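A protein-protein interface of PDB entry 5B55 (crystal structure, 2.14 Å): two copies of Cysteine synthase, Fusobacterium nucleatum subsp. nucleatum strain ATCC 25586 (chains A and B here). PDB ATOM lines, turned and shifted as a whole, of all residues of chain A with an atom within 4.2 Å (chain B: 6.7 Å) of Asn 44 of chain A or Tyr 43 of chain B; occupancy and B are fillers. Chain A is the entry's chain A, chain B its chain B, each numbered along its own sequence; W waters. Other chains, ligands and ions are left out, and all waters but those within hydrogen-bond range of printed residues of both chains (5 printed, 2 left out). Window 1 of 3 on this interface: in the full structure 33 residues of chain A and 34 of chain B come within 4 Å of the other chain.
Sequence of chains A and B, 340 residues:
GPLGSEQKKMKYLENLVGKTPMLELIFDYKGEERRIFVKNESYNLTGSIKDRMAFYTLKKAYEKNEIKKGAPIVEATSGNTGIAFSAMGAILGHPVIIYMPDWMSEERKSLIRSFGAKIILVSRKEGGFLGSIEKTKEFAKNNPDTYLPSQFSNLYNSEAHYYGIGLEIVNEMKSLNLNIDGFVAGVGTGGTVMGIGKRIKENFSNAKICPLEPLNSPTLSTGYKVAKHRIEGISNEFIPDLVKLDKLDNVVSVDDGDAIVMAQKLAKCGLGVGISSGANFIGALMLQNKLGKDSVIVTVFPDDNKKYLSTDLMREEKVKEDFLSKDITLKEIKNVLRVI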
ATOM      1  N   LEU A  16      20.630  -0.878  -4.080  1.00  0.00           N
ATOM      2  CA  LEU A  16      20.850   0.553  -3.913  1.00  0.00           C
ATOM      3  C   LEU A  16      21.597   1.200  -5.060  1.00  0.00           C
ATOM      4  O   LEU A  16      21.696   2.440  -5.092  1.00  0.00           O
ATOM      5  CB  LEU A  16      21.643   0.817  -2.609  1.00  0.00           C
ATOM      6  CG  LEU A  16      20.907   0.371  -1.325  1.00  0.00           C
ATOM      7  CD1 LEU A  16      21.816   0.587  -0.110  1.00  0.00           C
ATOM      8  CD2 LEU A  16      19.587   1.102  -1.104  1.00  0.00           C
ATOM      9  N   VAL A  17      22.152   0.394  -5.980  1.00  0.00           N
ATOM     10  CA  VAL A  17      22.908   0.904  -7.118  1.00  0.00           C
ATOM     11  C   VAL A  17      22.420   0.291  -8.445  1.00  0.00           C
ATOM     12  O   VAL A  17      21.791  -0.745  -8.460  1.00  0.00           O
ATOM     13  CB  VAL A  17      24.412   0.711  -6.966  1.00  0.00           C
ATOM     14  CG1 VAL A  17      24.847   1.326  -5.644  1.00  0.00           C
ATOM     15  CG2 VAL A  17      24.769  -0.767  -7.082  1.00  0.00           C
ATOM     16  N   GLY A  18      22.647   1.025  -9.526  1.00  0.00           N
ATOM     17  CA  GLY A  18      22.419   0.519 -10.827  1.00  0.00           C
ATOM     18  C   GLY A  18      20.962   0.492 -11.229  1.00  0.00           C
ATOM     19  O   GLY A  18      20.083   1.111 -10.607  1.00  0.00           O
ATOM     20  N   THR A  20      19.617   1.801 -13.935  1.00  0.00           N
ATOM     21  CA  THR A  20      19.294   3.184 -14.164  1.00  0.00           C
ATOM     22  C   THR A  20      18.623   3.337 -15.521  1.00  0.00           C
ATOM     23  O   THR A  20      18.771   2.467 -16.397  1.00  0.00           O
ATOM     24  CB  THR A  20      20.551   3.993 -14.207  1.00  0.00           C
ATOM     25  OG1 THR A  20      21.427   3.435 -15.203  1.00  0.00           O
ATOM     26  CG2 THR A  20      21.256   3.981 -12.809  1.00  0.00           C
ATOM     27  N   GLU A  41      22.935   8.327 -14.606  1.00  0.00           N
ATOM     28  CA  GLU A  41      23.504   7.724 -13.405  1.00  0.00           C
ATOM     29  C   GLU A  41      23.260   8.468 -12.103  1.00  0.00           C
ATOM     30  O   GLU A  41      23.815   8.102 -11.056  1.00  0.00           O
ATOM     31  CB  GLU A  41      24.963   7.394 -13.631  1.00  0.00           C
ATOM     32  CG  GLU A  41      25.154   6.370 -14.717  1.00  0.00           C
ATOM     33  CD  GLU A  41      24.594   5.002 -14.289  1.00  0.00           C
ATOM     34  OE1 GLU A  41      24.913   4.604 -13.176  1.00  0.00           O
ATOM     35  OE2 GLU A  41      23.889   4.316 -15.090  1.00  0.00           O
ATOM     36  N   SER A  42      22.354   9.448 -12.133  1.00  0.00           N
ATOM     37  CA  SER A  42      21.905  10.075 -10.901  1.00  0.00           C
ATOM     38  C   SER A  42      21.058   9.122 -10.015  1.00  0.00           C
ATOM     39  O   SER A  42      20.943   9.302  -8.770  1.00  0.00           O
ATOM     40  CB  SER A  42      21.210  11.418 -11.233  1.00  0.00           C
ATOM     41  OG  SER A  42      19.887  11.141 -11.657  1.00  0.00           O
ATOM     42  N   TYR A  43      20.480   8.080 -10.648  1.00  0.00           N
ATOM     43  CA  TYR A  43      19.564   7.204  -9.991  1.00  0.00           C
ATOM     44  C   TYR A  43      20.281   6.093  -9.180  1.00  0.00           C
ATOM     45  O   TYR A  43      20.133   4.865  -9.440  1.00  0.00           O
ATOM     46  CB  TYR A  43      18.584   6.585 -10.994  1.00  0.00           C
ATOM     47  CG  TYR A  43      17.573   7.461 -11.669  1.00  0.00           C
ATOM     48  CD1 TYR A  43      17.948   8.408 -12.629  1.00  0.00           C
ATOM     49  CD2 TYR A  43      16.214   7.265 -11.449  1.00  0.00           C
ATOM     50  CE1 TYR A  43      16.978   9.177 -13.293  1.00  0.00           C
ATOM     51  CE2 TYR A  43      15.267   8.047 -12.082  1.00  0.00           C
ATOM     52  CZ  TYR A  43      15.659   8.968 -13.026  1.00  0.00           C
ATOM     53  OH  TYR A  43      14.709   9.663 -13.698  1.00  0.00           O
ATOM     54  N   ASN A  44      21.031   6.563  -8.182  1.00  0.00           N
ATOM     55  CA  ASN A  44      21.983   5.778  -7.431  1.00  0.00           C
ATOM     56  C   ASN A  44      22.047   6.333  -6.036  1.00  0.00           C
ATOM     57  O   ASN A  44      21.691   7.485  -5.818  1.00  0.00           O
ATOM     58  CB  ASN A  44      23.384   5.800  -8.077  1.00  0.00           C
ATOM     59  CG  ASN A  44      23.559   4.776  -9.206  1.00  0.00           C
ATOM     60  OD1 ASN A  44      23.546   3.578  -8.968  1.00  0.00           O
ATOM     61  ND2 ASN A  44      23.821   5.253 -10.420  1.00  0.00           N
ATOM     62  N   LEU A  45      22.477   5.492  -5.093  1.00  0.00           N
ATOM     63  CA  LEU A  45      22.577   5.843  -3.660  1.00  0.00           C
ATOM     64  C   LEU A  45      22.960   7.295  -3.342  1.00  0.00           C
ATOM     65  O   LEU A  45      22.237   7.976  -2.596  1.00  0.00           O
ATOM     66  CB  LEU A  45      23.563   4.901  -2.927  1.00  0.00           C
ATOM     67  CG  LEU A  45      23.637   5.096  -1.391  1.00  0.00           C
ATOM     68  CD1 LEU A  45      22.259   4.874  -0.763  1.00  0.00           C
ATOM     69  CD2 LEU A  45      24.671   4.195  -0.786  1.00  0.00           C
ATOM     70  N   THR A  46      24.095   7.752  -3.844  1.00  0.00           N
ATOM     71  CA  THR A  46      24.570   9.126  -3.592  1.00  0.00           C
ATOM     72  C   THR A  46      24.508   9.991  -4.825  1.00  0.00           C
ATOM     73  O   THR A  46      25.035  11.108  -4.829  1.00  0.00           O
ATOM     74  CB  THR A  46      25.984   9.155  -3.020  1.00  0.00           C
ATOM     75  OG1 THR A  46      26.975   8.654  -3.964  1.00  0.00           O
ATOM     76  CG2 THR A  46      26.050   8.343  -1.733  1.00  0.00           C
ATOM     77  N   GLY A  47      23.812   9.519  -5.863  1.00  0.00           N
ATOM     78  CA  GLY A  47      23.605  10.288  -7.060  1.00  0.00           C
ATOM     79  C   GLY A  47      24.635  10.224  -8.205  1.00  0.00           C
ATOM     80  O   GLY A  47      24.651  11.120  -9.080  1.00  0.00           O
ATOM     81  N   SER A  48      25.486   9.223  -8.241  1.00  0.00           N
ATOM     82  CA  SER A  48      26.500   9.152  -9.289  1.00  0.00           C
ATOM     83  C   SER A  48      26.811   7.703  -9.650  1.00  0.00           C
ATOM     84  O   SER A  48      26.555   6.772  -8.875  1.00  0.00           O
ATOM     85  CB  SER A  48      27.765   9.864  -8.844  1.00  0.00           C
ATOM     86  OG  SER A  48      28.705   9.018  -8.231  1.00  0.00           O
ATOM     87  N   ASP A  51      28.700   5.226  -7.269  1.00  0.00           N
ATOM     88  CA  ASP A  51      28.124   4.264  -6.323  1.00  0.00           C
ATOM     89  C   ASP A  51      28.295   2.806  -6.763  1.00  0.00           C
ATOM     90  O   ASP A  51      28.454   1.908  -5.922  1.00  0.00           O
ATOM     91  CB  ASP A  51      26.669   4.560  -6.076  1.00  0.00           C
ATOM     92  CG  ASP A  51      26.450   5.928  -5.443  1.00  0.00           C
ATOM     93  OD1 ASP A  51      27.225   6.322  -4.533  1.00  0.00           O
ATOM     94  OD2 ASP A  51      25.485   6.603  -5.857  1.00  0.00           O
ATOM     95  N   ARG A  52      28.182   2.557  -8.080  1.00  0.00           N
ATOM     96  CA  ARG A  52      28.295   1.207  -8.613  1.00  0.00           C
ATOM     97  C   ARG A  52      29.677   0.658  -8.345  1.00  0.00           C
ATOM     98  O   ARG A  52      29.836  -0.552  -8.034  1.00  0.00           O
ATOM     99  CB  ARG A  52      28.080   1.170 -10.121  1.00  0.00           C
ATOM    100  CG  ARG A  52      26.668   1.552 -10.582  1.00  0.00           C
ATOM    101  CD  ARG A  52      26.718   1.723 -12.069  1.00  0.00           C
ATOM    102  NE  ARG A  52      25.488   2.035 -12.764  1.00  0.00           N
ATOM    103  CZ  ARG A  52      24.657   1.155 -13.303  1.00  0.00           C
ATOM    104  NH1 ARG A  52      24.814  -0.158 -13.101  1.00  0.00           N
ATOM    105  NH2 ARG A  52      23.594   1.613 -13.984  1.00  0.00           N
ATOM    106  N   LEU B  16      11.169   7.041 -15.710  1.00  0.00           N
ATOM    107  CA  LEU B  16      11.969   8.050 -15.027  1.00  0.00           C
ATOM    108  C   LEU B  16      11.584   8.281 -13.557  1.00  0.00           C
ATOM    109  O   LEU B  16      12.278   9.042 -12.865  1.00  0.00           O
ATOM    110  CB  LEU B  16      11.838   9.404 -15.775  1.00  0.00           C
ATOM    111  CG  LEU B  16      12.360   9.402 -17.203  1.00  0.00           C
ATOM    112  CD1 LEU B  16      12.093  10.742 -17.905  1.00  0.00           C
ATOM    113  CD2 LEU B  16      13.842   9.055 -17.306  1.00  0.00           C
ATOM    114  N   VAL B  17      10.459   7.715 -13.120  1.00  0.00           N
ATOM    115  CA  VAL B  17       9.976   7.928 -11.754  1.00  0.00           C
ATOM    116  C   VAL B  17       9.651   6.596 -11.084  1.00  0.00           C
ATOM    117  O   VAL B  17       9.405   5.602 -11.773  1.00  0.00           O
ATOM    118  CB  VAL B  17       8.790   8.869 -11.661  1.00  0.00           C
ATOM    119  CG1 VAL B  17       9.131  10.160 -12.345  1.00  0.00           C
ATOM    120  CG2 VAL B  17       7.514   8.236 -12.281  1.00  0.00           C
ATOM    121  N   GLY B  18       9.694   6.586  -9.754  1.00  0.00           N
ATOM    122  CA  GLY B  18       9.273   5.456  -9.023  1.00  0.00           C
ATOM    123  C   GLY B  18      10.232   4.269  -9.072  1.00  0.00           C
ATOM    124  O   GLY B  18      11.420   4.389  -9.433  1.00  0.00           O
ATOM    125  N   MLY B  19       9.700   3.146  -8.591  1.00  0.00           N
ATOM    126  CA  MLY B  19      10.412   1.889  -8.458  1.00  0.00           C
ATOM    127  CB  MLY B  19      10.794   1.297  -9.853  1.00  0.00           C
ATOM    128  CG  MLY B  19       9.684   1.297 -10.922  1.00  0.00           C
ATOM    129  CD  MLY B  19       8.531   0.417 -10.546  1.00  0.00           C
ATOM    130  CE  MLY B  19       7.585   0.057 -11.756  1.00  0.00           C
ATOM    131  NZ  MLY B  19       6.269  -0.689 -11.390  1.00  0.00           N
ATOM    132  CH1 MLY B  19       6.553  -1.777 -10.419  1.00  0.00           C
ATOM    133  CH2 MLY B  19       5.649  -1.251 -12.612  1.00  0.00           C
ATOM    134  C   MLY B  19      11.647   2.055  -7.563  1.00  0.00           C
ATOM    135  O   MLY B  19      12.731   1.599  -7.887  1.00  0.00           O
ATOM    136  N   THR B  20      11.451   2.699  -6.437  1.00  0.00           N
ATOM    137  CA  THR B  20      12.535   3.093  -5.569  1.00  0.00           C
ATOM    138  C   THR B  20      12.804   2.022  -4.528  1.00  0.00           C
ATOM    139  O   THR B  20      11.951   1.204  -4.244  1.00  0.00           O
ATOM    140  CB  THR B  20      12.135   4.361  -4.832  1.00  0.00           C
ATOM    141  OG1 THR B  20      10.906   4.084  -4.119  1.00  0.00           O
ATOM    142  CG2 THR B  20      11.940   5.524  -5.811  1.00  0.00           C
ATOM    143  N   PRO B  21      13.957   2.080  -3.879  1.00  0.00           N
ATOM    144  CA  PRO B  21      14.240   1.098  -2.856  1.00  0.00           C
ATOM    145  C   PRO B  21      13.385   1.254  -1.618  1.00  0.00           C
ATOM    146  O   PRO B  21      13.082   2.375  -1.215  1.00  0.00           O
ATOM    147  CB  PRO B  21      15.686   1.383  -2.451  1.00  0.00           C
ATOM    148  CG  PRO B  21      16.253   2.224  -3.561  1.00  0.00           C
ATOM    149  CD  PRO B  21      15.113   2.963  -4.154  1.00  0.00           C
ATOM    150  N   LEU B  23      13.775   0.167   2.205  1.00  0.00           N
ATOM    151  CA  LEU B  23      14.799  -0.219   3.146  1.00  0.00           C
ATOM    152  C   LEU B  23      14.199  -0.705   4.479  1.00  0.00           C
ATOM    153  O   LEU B  23      13.223  -0.120   4.975  1.00  0.00           O
ATOM    154  CB  LEU B  23      15.715   0.977   3.432  1.00  0.00           C
ATOM    155  CG  LEU B  23      16.152   1.767   2.206  1.00  0.00           C
ATOM    156  CD1 LEU B  23      16.231   3.252   2.577  1.00  0.00           C
ATOM    157  CD2 LEU B  23      17.485   1.317   1.790  1.00  0.00           C
ATOM    158  N   ASN B  40      13.020   5.184  -0.231  1.00  0.00           N
ATOM    159  CA  ASN B  40      14.037   6.157  -0.494  1.00  0.00           C
ATOM    160  C   ASN B  40      13.735   6.893  -1.833  1.00  0.00           C
ATOM    161  O   ASN B  40      14.086   6.419  -2.919  1.00  0.00           O
ATOM    162  CB  ASN B  40      15.417   5.498  -0.514  1.00  0.00           C
ATOM    163  CG  ASN B  40      16.527   6.538  -0.549  1.00  0.00           C
ATOM    164  OD1 ASN B  40      16.314   7.648  -0.983  1.00  0.00           O
ATOM    165  ND2 ASN B  40      17.688   6.184  -0.067  1.00  0.00           N
ATOM    166  N   GLU B  41      13.123   8.061  -1.736  1.00  0.00           N
ATOM    167  CA  GLU B  41      12.581   8.717  -2.908  1.00  0.00           C
ATOM    168  C   GLU B  41      13.520   9.647  -3.636  1.00  0.00           C
ATOM    169  O   GLU B  41      13.098  10.378  -4.540  1.00  0.00           O
ATOM    170  CB  GLU B  41      11.242   9.368  -2.567  1.00  0.00           C
ATOM    171  CG  GLU B  41      10.210   8.330  -2.166  1.00  0.00           C
ATOM    172  CD  GLU B  41       9.791   7.475  -3.324  1.00  0.00           C
ATOM    173  OE1 GLU B  41       9.544   8.051  -4.395  1.00  0.00           O
ATOM    174  OE2 GLU B  41       9.713   6.205  -3.197  1.00  0.00           O
ATOM    175  N   SER B  42      14.808   9.579  -3.297  1.00  0.00           N
ATOM    176  CA  SER B  42      15.835  10.309  -4.040  1.00  0.00           C
ATOM    177  C   SER B  42      16.069   9.691  -5.429  1.00  0.00           C
ATOM    178  O   SER B  42      16.506  10.380  -6.394  1.00  0.00           O
ATOM    179  CB  SER B  42      17.128  10.411  -3.207  1.00  0.00           C
ATOM    180  OG  SER B  42      17.840   9.201  -3.303  1.00  0.00           O
ATOM    181  N   TYR B  43      15.656   8.420  -5.565  1.00  0.00           N
ATOM    182  CA  TYR B  43      15.885   7.690  -6.787  1.00  0.00           C
ATOM    183  C   TYR B  43      14.820   7.982  -7.892  1.00  0.00           C
ATOM    184  O   TYR B  43      14.059   7.067  -8.370  1.00  0.00           O
ATOM    185  CB  TYR B  43      15.968   6.201  -6.504  1.00  0.00           C
ATOM    186  CG  TYR B  43      17.130   5.683  -5.730  1.00  0.00           C
ATOM    187  CD1 TYR B  43      17.251   5.916  -4.364  1.00  0.00           C
ATOM    188  CD2 TYR B  43      18.015   4.774  -6.314  1.00  0.00           C
ATOM    189  CE1 TYR B  43      18.284   5.332  -3.635  1.00  0.00           C
ATOM    190  CE2 TYR B  43      19.043   4.202  -5.612  1.00  0.00           C
ATOM    191  CZ  TYR B  43      19.164   4.453  -4.261  1.00  0.00           C
ATOM    192  OH  TYR B  43      20.152   3.864  -3.550  1.00  0.00           O
ATOM    193  N   ASN B  44      14.750   9.255  -8.254  1.00  0.00           N
ATOM    194  CA  ASN B  44      13.730   9.830  -9.084  1.00  0.00           C
ATOM    195  C   ASN B  44      14.346  10.896  -9.955  1.00  0.00           C
ATOM    196  O   ASN B  44      15.410  11.414  -9.619  1.00  0.00           O
ATOM    197  CB  ASN B  44      12.572  10.417  -8.251  1.00  0.00           C
ATOM    198  CG  ASN B  44      11.535   9.376  -7.848  1.00  0.00           C
ATOM    199  OD1 ASN B  44      10.821   8.843  -8.688  1.00  0.00           O
ATOM    200  ND2 ASN B  44      11.381   9.160  -6.554  1.00  0.00           N
ATOM    201  N   LEU B  45      13.701  11.206 -11.070  1.00  0.00           N
ATOM    202  CA  LEU B  45      14.186  12.267 -12.053  1.00  0.00           C
ATOM    203  C   LEU B  45      14.906  13.471 -11.508  1.00  0.00           C
ATOM    204  O   LEU B  45      16.048  13.762 -11.898  1.00  0.00           O
ATOM    205  CB  LEU B  45      13.039  12.770 -12.942  1.00  0.00           C
ATOM    206  CG  LEU B  45      13.441  13.692 -14.106  1.00  0.00           C
ATOM    207  CD1 LEU B  45      14.420  13.025 -15.043  1.00  0.00           C
ATOM    208  CD2 LEU B  45      12.237  14.192 -14.832  1.00  0.00           C
ATOM    209  N   GLY B  47      15.146  13.898  -8.053  1.00  0.00           N
ATOM    210  CA  GLY B  47      15.565  13.573  -6.678  1.00  0.00           C
ATOM    211  C   GLY B  47      14.519  13.610  -5.553  1.00  0.00           C
ATOM    212  O   GLY B  47      14.876  13.609  -4.372  1.00  0.00           O
ATOM    213  N   SER B  48      13.242  13.628  -5.890  1.00  0.00           N
ATOM    214  CA  SER B  48      12.233  13.632  -4.871  1.00  0.00           C
ATOM    215  C   SER B  48      10.998  12.844  -5.231  1.00  0.00           C
ATOM    216  O   SER B  48      10.701  12.595  -6.426  1.00  0.00           O
ATOM    217  CB  SER B  48      11.835  15.085  -4.517  1.00  0.00           C
ATOM    218  OG  SER B  48      10.742  15.529  -5.283  1.00  0.00           O
ATOM    219  N   ASP B  51       8.491  14.014  -8.099  1.00  0.00           N
ATOM    220  CA  ASP B  51       8.489  13.609  -9.493  1.00  0.00           C
ATOM    221  C   ASP B  51       7.319  12.663  -9.842  1.00  0.00           C
ATOM    222  O   ASP B  51       6.814  12.704 -10.985  1.00  0.00           O
ATOM    223  CB  ASP B  51       9.814  12.937  -9.886  1.00  0.00           C
ATOM    224  CG  ASP B  51      11.014  13.863  -9.731  1.00  0.00           C
ATOM    225  OD1 ASP B  51      10.919  15.065 -10.088  1.00  0.00           O
ATOM    226  OD2 ASP B  51      12.049  13.395  -9.228  1.00  0.00           O
ATOM    227  N   ARG B  52       6.991  11.734  -8.919  1.00  0.00           N
ATOM    228  CA  ARG B  52       5.898  10.762  -9.177  1.00  0.00           C
ATOM    229  C   ARG B  52       4.567  11.467  -9.363  1.00  0.00           C
ATOM    230  O   ARG B  52       3.777  11.119 -10.234  1.00  0.00           O
ATOM    231  CB  ARG B  52       5.728   9.821  -8.003  1.00  0.00           C
ATOM    232  CG  ARG B  52       6.895   8.910  -7.770  1.00  0.00           C
ATOM    233  CD  ARG B  52       6.654   8.247  -6.467  1.00  0.00           C
ATOM    234  NE  ARG B  52       7.601   7.273  -6.009  1.00  0.00           N
ATOM    235  CZ  ARG B  52       7.495   5.945  -6.192  1.00  0.00           C
ATOM    236  NH1 ARG B  52       6.566   5.427  -6.970  1.00  0.00           N
ATOM    237  NH2 ARG B  52       8.405   5.155  -5.656  1.00  0.00           N
ATOM    238  N   LEU B 271      22.763   7.214   4.351  1.00  0.00           N
ATOM    239  CA  LEU B 271      21.497   7.614   3.834  1.00  0.00           C
ATOM    240  C   LEU B 271      21.388   9.148   3.959  1.00  0.00           C
ATOM    241  O   LEU B 271      20.970   9.699   4.968  1.00  0.00           O
ATOM    242  CB  LEU B 271      20.361   6.907   4.528  1.00  0.00           C
ATOM    243  CG  LEU B 271      20.431   5.378   4.437  1.00  0.00           C
ATOM    244  CD1 LEU B 271      19.326   4.744   5.284  1.00  0.00           C
ATOM    245  CD2 LEU B 271      20.301   4.897   2.992  1.00  0.00           C
ATOM    246  N   ASP B 304      16.934  13.838  -1.026  1.00  0.00           N
ATOM    247  CA  ASP B 304      18.257  13.639  -0.458  1.00  0.00           C
ATOM    248  C   ASP B 304      18.731  14.901   0.275  1.00  0.00           C
ATOM    249  O   ASP B 304      17.978  15.848   0.392  1.00  0.00           O
ATOM    250  CB  ASP B 304      19.280  13.081  -1.491  1.00  0.00           C
ATOM    251  CG  ASP B 304      19.771  14.110  -2.542  1.00  0.00           C
ATOM    252  OD1 ASP B 304      19.627  15.368  -2.411  1.00  0.00           O
ATOM    253  OD2 ASP B 304      20.413  13.584  -3.532  1.00  0.00           O
ATOM    254  N   MLY B 306      21.194  17.003  -0.700  1.00  0.00           N
ATOM    255  CA  MLY B 306      21.948  17.893  -1.554  1.00  0.00           C
ATOM    256  CB  MLY B 306      22.114  17.355  -2.950  1.00  0.00           C
ATOM    257  CG  MLY B 306      22.953  16.062  -3.024  1.00  0.00           C
ATOM    258  CD  MLY B 306      23.350  15.793  -4.437  1.00  0.00           C
ATOM    259  CE  MLY B 306      24.207  14.551  -4.579  1.00  0.00           C
ATOM    260  NZ  MLY B 306      23.496  13.298  -4.166  1.00  0.00           N
ATOM    261  C   MLY B 306      21.399  19.321  -1.573  1.00  0.00           C
ATOM    262  O   MLY B 306      22.195  20.258  -1.599  1.00  0.00           O
ATOM    263  N   ARG B 338      13.768  -3.898  -4.144  1.00  0.00           N
ATOM    264  CA  ARG B 338      13.622  -3.080  -5.323  1.00  0.00           C
ATOM    265  C   ARG B 338      12.871  -3.917  -6.335  1.00  0.00           C
ATOM    266  O   ARG B 338      13.439  -4.901  -6.840  1.00  0.00           O
ATOM    267  CB  ARG B 338      15.038  -2.683  -5.812  1.00  0.00           C
ATOM    268  CG  ARG B 338      15.137  -1.561  -6.834  1.00  0.00           C
ATOM    269  CD  ARG B 338      15.386  -0.216  -6.185  1.00  0.00           C
ATOM    270  NE  ARG B 338      15.390   0.899  -7.150  1.00  0.00           N
ATOM    271  CZ  ARG B 338      16.473   1.498  -7.654  1.00  0.00           C
ATOM    272  NH1 ARG B 338      17.711   1.089  -7.366  1.00  0.00           N
ATOM    273  NH2 ARG B 338      16.300   2.523  -8.491  1.00  0.00           N
HETATM  274  O   HOH W   1      18.128  11.527  -9.568  1.00  0.00           O
HETATM  275  O   HOH W   2      19.493  11.654  -7.113  1.00  0.00           O
HETATM  276  O   HOH W   3      17.905  12.931 -13.784  1.00  0.00           O
HETATM  277  O   HOH W   4      19.734   9.330  -5.085  1.00  0.00           O
HETATM  278  O   HOH W   5      18.142   3.243 -10.677  1.00  0.00           O
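N of Gly 18 of chain A sits at hydrogen-bond distance from OD1 of Asn 44 of chain A, 2.8 Å away.
O of Glu 41 of chain A is in hydrogen-bond range of ND2 of Asn 44 of chain A, 2.9 Å away.
The backbone carbonyl oxygen (O) of Ser 48 of chain A sits close to the side-chain amide nitrogen (ND2) of Asn 44 of chain A (3.5 Å).
The backbone NH of Leu 45 of chain A sits at hydrogen-bond distance from the side-chain carboxylate of Asp 51 of chain A, at 3.3 Å.
The backbone carbonyl oxygen of Leu 16 of chain B lies within hydrogen-bond range of the backbone NH of Leu 45 of chain B (3.2 Å).
ND2 of Asn 44 of chain B is in hydrogen-bond range of O of Glu 41 of chain B (2.9 Å).
Printed residues of chain B within 4 Å of Tyr 43 of chain A: Leu 16 (2.6 Å), Tyr 43 (3.8 Å), Asn 44 (3.7 Å) and Leu 45 (3.1 Å).
Asn 44 of chain A touches just one residue of chain B: Tyr 43 (3.7 Å).
Printed residues of chain B within 4 Å of Leu 45 of chain A: Tyr 43.
Of the printed residues of chain A, Leu 16 of chain B touches Tyr 43.
MLY 19 of chain B touches none of the printed residues of chain A.
Of the printed residues of chain A, Tyr 43 of chain B touches Leu 16 (2.6 Å), Tyr 43 (3.8 Å), Asn 44 (3.7 Å) and Leu 45 (3.1 Å).
Printed residues of chain A within 4 Å of Asn 44 of chain B: Tyr 43.
The nearest residue of chain B that does not touch Asn 44 of chain A is Ser 42 of chain B (4.9 Å).
The nearest printed residue of chain A that does not touch Tyr 43 of chain B is Val 17 of chain A (4.7 Å).
Among the printed residues, merely in contact across the chains: Leu 16 of chain A with Leu 23 of chain B (3.6 Å), Tyr 43 of chain A with Tyr 43 of chain B (3.8 Å), Tyr 43 of chain A with Asn 44 of chain B (3.7 Å) and Asn 44 of chain A with Tyr 43 of chain B (3.7 Å).
Leu 16 of chain A touches Tyr 43 of chain B, and with the chains exchanged Tyr 43 of chain A touches Leu 16 of chain B.
Tyr 43 of chain B touches its own counterpart, Tyr 43 of chain A.
Tyr 43 of chain A touches Asn 44 of chain B, and with the chains exchanged Asn 44 of chain A touches Tyr 43 of chain B.
Tyr 43 of chain A touches Leu 45 of chain B, and with the chains exchanged Leu 45 of chain A touches Tyr 43 of chain B.
Positions printed for both chains: 16, 17, 18, 20, 41, 42, 43, 44, 45, 47, 48, 51 and 52.
Of the 9 pairs that touch across the chains among the printed residues, 7 have their exchanged pair printed and touching as well.
Of the 21 printed residues of chain B, 6 touch a printed residue of chain A.
Hydrophobic or aromatic side chains of chain B within 4 Å of the printed part of chain A: Leu 16, Leu 23, Tyr 43 and Leu 45.
Of the 14 printed residues of chain A, 5 touch a printed residue of chain B.
Hydrophobic or aromatic side chains of chain A within 4 Å of the printed part of chain B: Leu 16, Tyr 43 and Leu 45.
Among the printed residues, 9 pairs touch across the chains.
O of Leu 16 of chain A is in hydrogen-bond range of OH of Tyr 43 of chain B, 2.6 Å away.
O of Leu 16 of chain B lies within hydrogen-bond range of OH of Tyr 43 of chain A, 2.6 Å away.
The backbone NH (N) of Leu 45 of chain B sits close to the side-chain hydroxyl (OH) of Tyr 43 of chain A, 3.2 Å away.
The backbone NH (N) of Leu 45 of chain A sits close to the side-chain hydroxyl (OH) of Tyr 43 of chain B.
NZ of MLY 306 of chain B sits close to O of Thr 46 of chain A, 2.8 Å away.
Water W4 bridges OG of Ser 42 of chain B and O of Asn 44 of chain A.
Water W1 bridges O of Asn 44 of chain B (2.7 Å) and OG of Ser 42 of chain A (2.8 Å).
Water W3 bridges the backbone carbonyl oxygen of Leu 45 of chain B (2.8 Å) and the side-chain hydroxyl of Ser 42 of chain A (3.4 Å).
Water W5 lies within hydrogen-bond range of the backbone carbonyl oxygen of Tyr 43 of chain A (2.9 Å), the backbone carbonyl oxygen of Gly 18 of chain A (2.9 Å) and the guanidinium group of Arg 338 of chain B (2.9 Å).
Water W2 lies within hydrogen-bond range of the backbone carbonyl oxygen of Ser 42 of chain A and the backbone carbonyl oxygen of Ser 42 of chain B.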
